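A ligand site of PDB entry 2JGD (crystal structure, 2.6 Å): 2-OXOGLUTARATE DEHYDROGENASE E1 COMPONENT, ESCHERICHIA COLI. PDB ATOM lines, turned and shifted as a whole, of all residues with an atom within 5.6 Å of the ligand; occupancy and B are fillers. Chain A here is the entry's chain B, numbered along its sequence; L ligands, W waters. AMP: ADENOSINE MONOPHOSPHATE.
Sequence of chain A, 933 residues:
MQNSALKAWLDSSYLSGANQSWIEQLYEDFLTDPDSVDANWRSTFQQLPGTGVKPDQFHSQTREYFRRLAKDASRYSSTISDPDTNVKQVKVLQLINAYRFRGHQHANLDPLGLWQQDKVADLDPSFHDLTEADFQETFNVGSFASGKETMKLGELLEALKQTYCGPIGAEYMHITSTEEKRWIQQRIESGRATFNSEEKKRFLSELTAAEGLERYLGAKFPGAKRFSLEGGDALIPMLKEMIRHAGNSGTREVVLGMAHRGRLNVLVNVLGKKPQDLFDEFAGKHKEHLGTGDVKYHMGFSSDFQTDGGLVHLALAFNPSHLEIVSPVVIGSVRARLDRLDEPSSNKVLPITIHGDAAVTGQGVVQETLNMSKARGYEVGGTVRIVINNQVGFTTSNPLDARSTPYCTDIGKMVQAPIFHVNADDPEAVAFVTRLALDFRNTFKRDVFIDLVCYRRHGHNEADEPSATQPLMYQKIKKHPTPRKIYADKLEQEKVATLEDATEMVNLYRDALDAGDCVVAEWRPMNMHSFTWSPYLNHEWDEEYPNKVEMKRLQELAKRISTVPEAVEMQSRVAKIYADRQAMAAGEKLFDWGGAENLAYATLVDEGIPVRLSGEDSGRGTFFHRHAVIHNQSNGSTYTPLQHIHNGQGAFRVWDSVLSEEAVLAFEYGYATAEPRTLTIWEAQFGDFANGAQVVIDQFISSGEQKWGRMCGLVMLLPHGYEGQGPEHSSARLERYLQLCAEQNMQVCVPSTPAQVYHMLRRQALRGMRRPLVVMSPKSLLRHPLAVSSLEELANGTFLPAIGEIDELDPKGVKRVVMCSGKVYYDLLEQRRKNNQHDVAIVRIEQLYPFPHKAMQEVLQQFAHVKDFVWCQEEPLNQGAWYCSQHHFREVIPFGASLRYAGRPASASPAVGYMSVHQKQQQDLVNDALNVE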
ATOM      1  N   GLU A 253      25.450 -26.151  13.423  1.00  0.00           N
ATOM      2  CA  GLU A 253      24.482 -26.835  14.252  1.00  0.00           C
ATOM      3  C   GLU A 253      24.131 -28.208  13.671  1.00  0.00           C
ATOM      4  O   GLU A 253      23.957 -28.356  12.467  1.00  0.00           O
ATOM      5  CB  GLU A 253      23.210 -26.000  14.403  1.00  0.00           C
ATOM      6  CG  GLU A 253      23.182 -25.040  15.603  1.00  0.00           C
ATOM      7  CD  GLU A 253      22.231 -23.845  15.394  1.00  0.00           C
ATOM      8  OE1 GLU A 253      21.130 -23.824  15.985  1.00  0.00           O
ATOM      9  OE2 GLU A 253      22.587 -22.926  14.625  1.00  0.00           O
ATOM     10  N   PHE A 301      18.673 -33.446  24.418  1.00  0.00           N
ATOM     11  CA  PHE A 301      19.851 -32.908  25.020  1.00  0.00           C
ATOM     12  C   PHE A 301      20.477 -31.899  24.086  1.00  0.00           C
ATOM     13  O   PHE A 301      20.405 -32.035  22.855  1.00  0.00           O
ATOM     14  CB  PHE A 301      20.833 -34.028  25.349  1.00  0.00           C
ATOM     15  CG  PHE A 301      21.796 -33.700  26.448  1.00  0.00           C
ATOM     16  CD1 PHE A 301      23.064 -33.201  26.160  1.00  0.00           C
ATOM     17  CD2 PHE A 301      21.437 -33.880  27.788  1.00  0.00           C
ATOM     18  CE1 PHE A 301      23.980 -32.894  27.191  1.00  0.00           C
ATOM     19  CE2 PHE A 301      22.332 -33.579  28.817  1.00  0.00           C
ATOM     20  CZ  PHE A 301      23.607 -33.060  28.509  1.00  0.00           C
ATOM     21  N   SER A 302      21.004 -30.834  24.674  1.00  0.00           N
ATOM     22  CA  SER A 302      21.714 -29.820  23.928  1.00  0.00           C
ATOM     23  C   SER A 302      23.129 -29.729  24.465  1.00  0.00           C
ATOM     24  O   SER A 302      23.371 -29.845  25.666  1.00  0.00           O
ATOM     25  CB  SER A 302      21.018 -28.469  24.099  1.00  0.00           C
ATOM     26  OG  SER A 302      19.644 -28.536  23.748  1.00  0.00           O
ATOM     27  N   SER A 303      24.067 -29.487  23.573  1.00  0.00           N
ATOM     28  CA  SER A 303      25.432 -29.363  23.981  1.00  0.00           C
ATOM     29  C   SER A 303      26.290 -28.822  22.832  1.00  0.00           C
ATOM     30  O   SER A 303      25.866 -28.810  21.674  1.00  0.00           O
ATOM     31  CB  SER A 303      25.947 -30.735  24.421  1.00  0.00           C
ATOM     32  OG  SER A 303      26.408 -31.468  23.302  1.00  0.00           O
ATOM     33  N   HIS A 313      27.164 -26.821  17.551  1.00  0.00           N
ATOM     34  CA  HIS A 313      26.039 -27.055  18.474  1.00  0.00           C
ATOM     35  C   HIS A 313      25.310 -28.339  18.127  1.00  0.00           C
ATOM     36  O   HIS A 313      25.021 -28.563  16.964  1.00  0.00           O
ATOM     37  CB  HIS A 313      25.043 -25.878  18.451  1.00  0.00           C
ATOM     38  CG  HIS A 313      23.973 -26.009  19.500  1.00  0.00           C
ATOM     39  ND1 HIS A 313      24.250 -26.057  20.837  1.00  0.00           N
ATOM     40  CD2 HIS A 313      22.636 -26.171  19.385  1.00  0.00           C
ATOM     41  CE1 HIS A 313      23.129 -26.217  21.514  1.00  0.00           C
ATOM     42  NE2 HIS A 313      22.128 -26.285  20.653  1.00  0.00           N
ATOM     43  N   LEU A 314      24.978 -29.138  19.134  1.00  0.00           N
ATOM     44  CA  LEU A 314      24.206 -30.382  18.940  1.00  0.00           C
ATOM     45  C   LEU A 314      22.884 -30.315  19.685  1.00  0.00           C
ATOM     46  O   LEU A 314      22.844 -30.034  20.897  1.00  0.00           O
ATOM     47  CB  LEU A 314      24.970 -31.590  19.504  1.00  0.00           C
ATOM     48  CG  LEU A 314      26.435 -31.739  19.127  1.00  0.00           C
ATOM     49  CD1 LEU A 314      26.999 -33.040  19.698  1.00  0.00           C
ATOM     50  CD2 LEU A 314      26.539 -31.691  17.599  1.00  0.00           C
ATOM     51  N   ALA A 315      21.808 -30.641  18.992  1.00  0.00           N
ATOM     52  CA  ALA A 315      20.495 -30.608  19.611  1.00  0.00           C
ATOM     53  C   ALA A 315      19.799 -31.893  19.273  1.00  0.00           C
ATOM     54  O   ALA A 315      19.531 -32.187  18.096  1.00  0.00           O
ATOM     55  CB  ALA A 315      19.680 -29.382  19.132  1.00  0.00           C
ATOM     56  N   SER A 333      12.605 -27.717  13.116  1.00  0.00           N
ATOM     57  CA  SER A 333      13.637 -27.128  13.924  1.00  0.00           C
ATOM     58  C   SER A 333      14.762 -26.566  13.038  1.00  0.00           C
ATOM     59  O   SER A 333      15.180 -25.409  13.185  1.00  0.00           O
ATOM     60  CB  SER A 333      14.189 -28.149  14.908  1.00  0.00           C
ATOM     61  OG  SER A 333      14.880 -27.511  15.972  1.00  0.00           O
ATOM     62  N   ARG A 337      16.338 -22.755  12.482  1.00  0.00           N
ATOM     63  CA  ARG A 337      17.743 -22.442  12.661  1.00  0.00           C
ATOM     64  C   ARG A 337      18.393 -21.819  11.425  1.00  0.00           C
ATOM     65  O   ARG A 337      19.256 -20.946  11.544  1.00  0.00           O
ATOM     66  CB  ARG A 337      18.513 -23.682  13.120  1.00  0.00           C
ATOM     67  CG  ARG A 337      18.105 -24.133  14.560  1.00  0.00           C
ATOM     68  CD  ARG A 337      18.441 -25.586  14.806  1.00  0.00           C
ATOM     69  NE  ARG A 337      17.630 -26.147  15.877  1.00  0.00           N
ATOM     70  CZ  ARG A 337      17.919 -26.030  17.168  1.00  0.00           C
ATOM     71  NH1 ARG A 337      18.997 -25.347  17.565  1.00  0.00           N
ATOM     72  NH2 ARG A 337      17.128 -26.576  18.072  1.00  0.00           N
ATOM     73  N   ARG A 340      17.397 -18.066  10.888  1.00  0.00           N
ATOM     74  CA  ARG A 340      18.053 -17.033  11.692  1.00  0.00           C
ATOM     75  C   ARG A 340      19.488 -16.763  11.313  1.00  0.00           C
ATOM     76  O   ARG A 340      20.183 -16.036  12.010  1.00  0.00           O
ATOM     77  CB  ARG A 340      17.967 -17.297  13.210  1.00  0.00           C
ATOM     78  CG  ARG A 340      18.075 -18.712  13.642  1.00  0.00           C
ATOM     79  CD  ARG A 340      18.577 -18.783  15.067  1.00  0.00           C
ATOM     80  NE  ARG A 340      17.658 -19.488  15.963  1.00  0.00           N
ATOM     81  CZ  ARG A 340      17.971 -20.600  16.641  1.00  0.00           C
ATOM     82  NH1 ARG A 340      19.170 -21.160  16.513  1.00  0.00           N
ATOM     83  NH2 ARG A 340      17.086 -21.139  17.459  1.00  0.00           N
ATOM     84  N   MET A 526      27.631 -24.660  26.919  1.00  0.00           N
ATOM     85  CA  MET A 526      27.210 -23.748  25.872  1.00  0.00           C
ATOM     86  C   MET A 526      27.466 -22.313  26.320  1.00  0.00           C
ATOM     87  O   MET A 526      27.530 -22.029  27.505  1.00  0.00           O
ATOM     88  CB  MET A 526      25.739 -23.934  25.523  1.00  0.00           C
ATOM     89  CG  MET A 526      25.359 -25.356  25.101  1.00  0.00           C
ATOM     90  SD  MET A 526      23.625 -25.712  25.411  1.00  0.00           S
ATOM     91  CE  MET A 526      22.863 -24.369  24.517  1.00  0.00           C
ATOM     92  N   SER A 530      23.626 -19.110  23.254  1.00  0.00           N
ATOM     93  CA  SER A 530      22.913 -20.312  22.861  1.00  0.00           C
ATOM     94  C   SER A 530      21.646 -20.561  23.630  1.00  0.00           C
ATOM     95  O   SER A 530      20.917 -21.506  23.333  1.00  0.00           O
ATOM     96  CB  SER A 530      23.820 -21.519  22.991  1.00  0.00           C
ATOM     97  OG  SER A 530      24.775 -21.532  21.944  1.00  0.00           O
ATOM     98  N   PHE A 531      21.365 -19.743  24.644  1.00  0.00           N
ATOM     99  CA  PHE A 531      20.142 -19.960  25.407  1.00  0.00           C
ATOM    100  C   PHE A 531      18.961 -19.120  24.922  1.00  0.00           C
ATOM    101  O   PHE A 531      18.552 -18.146  25.545  1.00  0.00           O
ATOM    102  CB  PHE A 531      20.403 -19.826  26.896  1.00  0.00           C
ATOM    103  CG  PHE A 531      21.276 -20.902  27.455  1.00  0.00           C
ATOM    104  CD1 PHE A 531      22.657 -20.737  27.504  1.00  0.00           C
ATOM    105  CD2 PHE A 531      20.724 -22.092  27.891  1.00  0.00           C
ATOM    106  CE1 PHE A 531      23.485 -21.752  27.987  1.00  0.00           C
ATOM    107  CE2 PHE A 531      21.554 -23.104  28.387  1.00  0.00           C
ATOM    108  CZ  PHE A 531      22.931 -22.932  28.421  1.00  0.00           C
ATOM    109  N   THR A 532      18.407 -19.513  23.791  1.00  0.00           N
ATOM    110  CA  THR A 532      17.521 -18.652  23.046  1.00  0.00           C
ATOM    111  C   THR A 532      16.176 -18.534  23.743  1.00  0.00           C
ATOM    112  O   THR A 532      15.375 -17.680  23.415  1.00  0.00           O
ATOM    113  CB  THR A 532      17.329 -19.187  21.622  1.00  0.00           C
ATOM    114  OG1 THR A 532      17.140 -20.602  21.676  1.00  0.00           O
ATOM    115  CG2 THR A 532      18.571 -18.902  20.778  1.00  0.00           C
ATOM    116  N   TRP A 533      15.955 -19.379  24.738  1.00  0.00           N
ATOM    117  CA  TRP A 533      14.649 -19.402  25.395  1.00  0.00           C
ATOM    118  C   TRP A 533      14.579 -18.707  26.736  1.00  0.00           C
ATOM    119  O   TRP A 533      13.496 -18.590  27.306  1.00  0.00           O
ATOM    120  CB  TRP A 533      14.127 -20.823  25.516  1.00  0.00           C
ATOM    121  CG  TRP A 533      13.583 -21.294  24.244  1.00  0.00           C
ATOM    122  CD1 TRP A 533      14.272 -21.861  23.224  1.00  0.00           C
ATOM    123  CD2 TRP A 533      12.248 -21.146  23.783  1.00  0.00           C
ATOM    124  NE1 TRP A 533      13.451 -22.115  22.174  1.00  0.00           N
ATOM    125  CE2 TRP A 533      12.194 -21.700  22.498  1.00  0.00           C
ATOM    126  CE3 TRP A 533      11.073 -20.657  24.356  1.00  0.00           C
ATOM    127  CZ2 TRP A 533      11.027 -21.763  21.767  1.00  0.00           C
ATOM    128  CZ3 TRP A 533       9.895 -20.733  23.630  1.00  0.00           C
ATOM    129  CH2 TRP A 533       9.889 -21.263  22.354  1.00  0.00           C
ATOM    130  N   LEU A 537      10.509 -17.889  29.604  1.00  0.00           N
ATOM    131  CA  LEU A 537      10.480 -19.170  30.299  1.00  0.00           C
ATOM    132  C   LEU A 537       9.339 -19.231  31.304  1.00  0.00           C
ATOM    133  O   LEU A 537       8.625 -20.237  31.387  1.00  0.00           O
ATOM    134  CB  LEU A 537      11.818 -19.420  31.010  1.00  0.00           C
ATOM    135  CG  LEU A 537      12.776 -20.396  30.320  1.00  0.00           C
ATOM    136  CD1 LEU A 537      13.504 -21.242  31.344  1.00  0.00           C
ATOM    137  CD2 LEU A 537      12.018 -21.281  29.333  1.00  0.00           C
ATOM    138  N   ALA A 672       8.392 -23.753  15.723  1.00  0.00           N
ATOM    139  CA  ALA A 672       8.104 -22.879  16.867  1.00  0.00           C
ATOM    140  C   ALA A 672       8.925 -23.171  18.121  1.00  0.00           C
ATOM    141  O   ALA A 672       9.221 -22.250  18.862  1.00  0.00           O
ATOM    142  CB  ALA A 672       6.659 -22.867  17.192  1.00  0.00           C
ATOM    143  N   THR A 673       9.250 -24.438  18.379  1.00  0.00           N
ATOM    144  CA  THR A 673      10.036 -24.756  19.586  1.00  0.00           C
ATOM    145  C   THR A 673      11.468 -24.285  19.405  1.00  0.00           C
ATOM    146  O   THR A 673      12.196 -24.142  20.352  1.00  0.00           O
ATOM    147  CB  THR A 673      10.079 -26.248  19.875  1.00  0.00           C
ATOM    148  OG1 THR A 673      10.419 -26.938  18.690  1.00  0.00           O
ATOM    149  CG2 THR A 673       8.728 -26.748  20.397  1.00  0.00           C
ATOM    150  N   ALA A 674      11.850 -24.013  18.168  1.00  0.00           N
ATOM    151  CA  ALA A 674      13.191 -23.550  17.866  1.00  0.00           C
ATOM    152  C   ALA A 674      13.296 -22.027  17.917  1.00  0.00           C
ATOM    153  O   ALA A 674      14.373 -21.490  18.151  1.00  0.00           O
ATOM    154  CB  ALA A 674      13.626 -24.050  16.500  1.00  0.00           C
ATOM    155  N   GLY A 709       9.547 -29.836  29.438  1.00  0.00           N
ATOM    156  CA  GLY A 709       9.879 -28.431  29.659  1.00  0.00           C
ATOM    157  C   GLY A 709       9.980 -27.623  28.379  1.00  0.00           C
ATOM    158  O   GLY A 709      10.645 -26.593  28.337  1.00  0.00           O
ATOM    159  N   ARG A 710       9.315 -28.095  27.340  1.00  0.00           N
ATOM    160  CA  ARG A 710       9.472 -27.508  26.015  1.00  0.00           C
ATOM    161  C   ARG A 710       8.351 -26.512  25.732  1.00  0.00           C
ATOM    162  O   ARG A 710       7.200 -26.908  25.611  1.00  0.00           O
ATOM    163  CB  ARG A 710       9.416 -28.623  24.981  1.00  0.00           C
ATOM    164  CG  ARG A 710      10.703 -29.325  24.869  1.00  0.00           C
ATOM    165  CD  ARG A 710      11.510 -28.635  23.849  1.00  0.00           C
ATOM    166  NE  ARG A 710      12.908 -28.748  24.126  1.00  0.00           N
ATOM    167  CZ  ARG A 710      13.816 -28.782  23.178  1.00  0.00           C
ATOM    168  NH1 ARG A 710      13.417 -28.726  21.905  1.00  0.00           N
ATOM    169  NH2 ARG A 710      15.109 -28.874  23.505  1.00  0.00           N
ATOM    170  N   MET A 711       8.683 -25.222  25.624  1.00  0.00           N
ATOM    171  CA  MET A 711       7.681 -24.197  25.410  1.00  0.00           C
ATOM    172  C   MET A 711       7.424 -24.103  23.909  1.00  0.00           C
ATOM    173  O   MET A 711       8.187 -24.611  23.121  1.00  0.00           O
ATOM    174  CB  MET A 711       8.155 -22.849  25.951  1.00  0.00           C
ATOM    175  CG  MET A 711       8.377 -22.828  27.446  1.00  0.00           C
ATOM    176  SD  MET A 711       7.180 -23.789  28.363  1.00  0.00           S
ATOM    177  CE  MET A 711       5.773 -22.685  28.280  1.00  0.00           C
ATOM    178  N   CYS A 712       6.329 -23.459  23.509  1.00  0.00           N
ATOM    179  CA  CYS A 712       5.967 -23.432  22.104  1.00  0.00           C
ATOM    180  C   CYS A 712       4.812 -22.457  21.882  1.00  0.00           C
ATOM    181  O   CYS A 712       3.730 -22.632  22.453  1.00  0.00           O
ATOM    182  CB  CYS A 712       5.585 -24.831  21.621  1.00  0.00           C
ATOM    183  SG  CYS A 712       4.765 -24.918  20.003  1.00  0.00           S
HETATM  184  P   AMP L   1      18.788 -25.897  21.224  1.00  0.00           P
HETATM  185  O1P AMP L   1      19.236 -24.715  20.371  1.00  0.00           O
HETATM  186  O2P AMP L   1      19.907 -26.860  21.603  1.00  0.00           O
HETATM  187  O3P AMP L   1      17.540 -26.600  20.772  1.00  0.00           O
HETATM  188  O5' AMP L   1      18.355 -25.195  22.613  1.00  0.00           O
HETATM  189  C5' AMP L   1      19.313 -24.397  23.332  1.00  0.00           C
HETATM  190  C4' AMP L   1      18.956 -24.319  24.817  1.00  0.00           C
HETATM  191  O4' AMP L   1      17.625 -23.811  24.962  1.00  0.00           O
HETATM  192  C3' AMP L   1      18.955 -25.678  25.491  1.00  0.00           C
HETATM  193  O3' AMP L   1      19.150 -25.468  26.891  1.00  0.00           O
HETATM  194  C2' AMP L   1      17.531 -26.126  25.354  1.00  0.00           C
HETATM  195  O2' AMP L   1      17.158 -27.011  26.426  1.00  0.00           O
HETATM  196  C1' AMP L   1      16.752 -24.825  25.468  1.00  0.00           C
HETATM  197  N9  AMP L   1      15.533 -24.913  24.641  1.00  0.00           N
HETATM  198  C8  AMP L   1      15.509 -25.152  23.317  1.00  0.00           C
HETATM  199  N7  AMP L   1      14.235 -25.196  22.865  1.00  0.00           N
HETATM  200  C5  AMP L   1      13.424 -24.998  23.920  1.00  0.00           C
HETATM  201  C6  AMP L   1      11.964 -24.944  24.117  1.00  0.00           C
HETATM  202  N6  AMP L   1      11.132 -25.067  23.053  1.00  0.00           N
HETATM  203  N1  AMP L   1      11.491 -24.738  25.373  1.00  0.00           N
HETATM  204  C2  AMP L   1      12.337 -24.573  26.412  1.00  0.00           C
HETATM  205  N3  AMP L   1      13.695 -24.623  26.291  1.00  0.00           N
HETATM  206  C4  AMP L   1      14.276 -24.825  25.095  1.00  0.00           C
HETATM  207  O   HOH W   1      14.980 -25.500  20.222  1.00  0.00           O
HETATM  208  O   HOH W   2      14.760 -23.992  29.046  1.00  0.00           O
HETATM  209  O   HOH W   3      21.240 -23.189  20.531  1.00  0.00           O
HETATM  210  O   HOH W   4      17.443 -22.907  19.664  1.00  0.00           O
HETATM  211  O   HOH W   5      17.562 -30.204  27.327  1.00  0.00           O
HETATM  212  O   HOH W   6      20.637 -27.260  27.780  1.00  0.00           O
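An oxygen (O2P) of the ligand lies within hydrogen-bond range of a ring nitrogen (NE2) of His 313 (2.5 Å). NH2 of Arg 337 is in salt-bridge range of O3P of the ligand (2.7 Å). OG of Ser 302 is in hydrogen-bond range of O2P of the ligand, at 2.7 Å. The backbone NH of Met 711 is in hydrogen-bond range of a nitrogen (N1) of the ligand. A nitrogen (N6) of the ligand is in hydrogen-bond range of the backbone carbonyl oxygen of Met 711, 3.0 Å away. N6 of the ligand lies within hydrogen-bond range of O of Thr 673 (3.0 Å). A nitrogen (N7) of the ligand is in hydrogen-bond range of the indole nitrogen (NE1) of Trp 533, at 3.3 Å.
Water W3 lies within hydrogen-bond range of an oxygen (O1P) of the ligand (2.5 Å), a ring nitrogen (NE2) of His 313 (3.2 Å) and the backbone carbonyl oxygen (O) of Ser 530 (3.3 Å). Water W4 lies within hydrogen-bond range of O1P of the ligand (2.6 Å), NH2 of Arg 340 (2.8 Å) and OG1 of Thr 532 (3.1 Å). Water W1 lies within hydrogen-bond range of N7 of the ligand (2.8 Å), O of Thr 673 (3.1 Å) and NH2 of Arg 337 (3.2 Å).
CB of Ala 315 touches O2P of the ligand, 3.5 Å away. Met 526 touches the ligand. Ser 530 touches the ligand. CE2 of Phe 531 touches O3' of the ligand, 3.7 Å away. O of Gly 709 touches C2 of the ligand (3.3 Å). Arg 710 touches the ligand (CA to N1, 3.5 Å). Hydrophobic or aromatic side chains that line the ligand: His 313, Ala 315, Met 526, Phe 531, Trp 533 and Met 711. The nearest printed residue that does not touch the ligand is Leu 314 (4.4 Å).
A ring nitrogen (ND1) of His 313 is in hydrogen-bond range of the backbone carbonyl oxygen (O) of Ser 303 (3.3 Å). NH1 of Arg 337 lies within salt-bridge range of OE1 of Glu 253. The side-chain hydroxyl of Ser 333 is in hydrogen-bond range of the guanidinium group of Arg 337, 3.1 Å away. The indole nitrogen (NE1) of Trp 533 lies within hydrogen-bond range of the backbone carbonyl oxygen (O) of Thr 673, 3.0 Å away.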
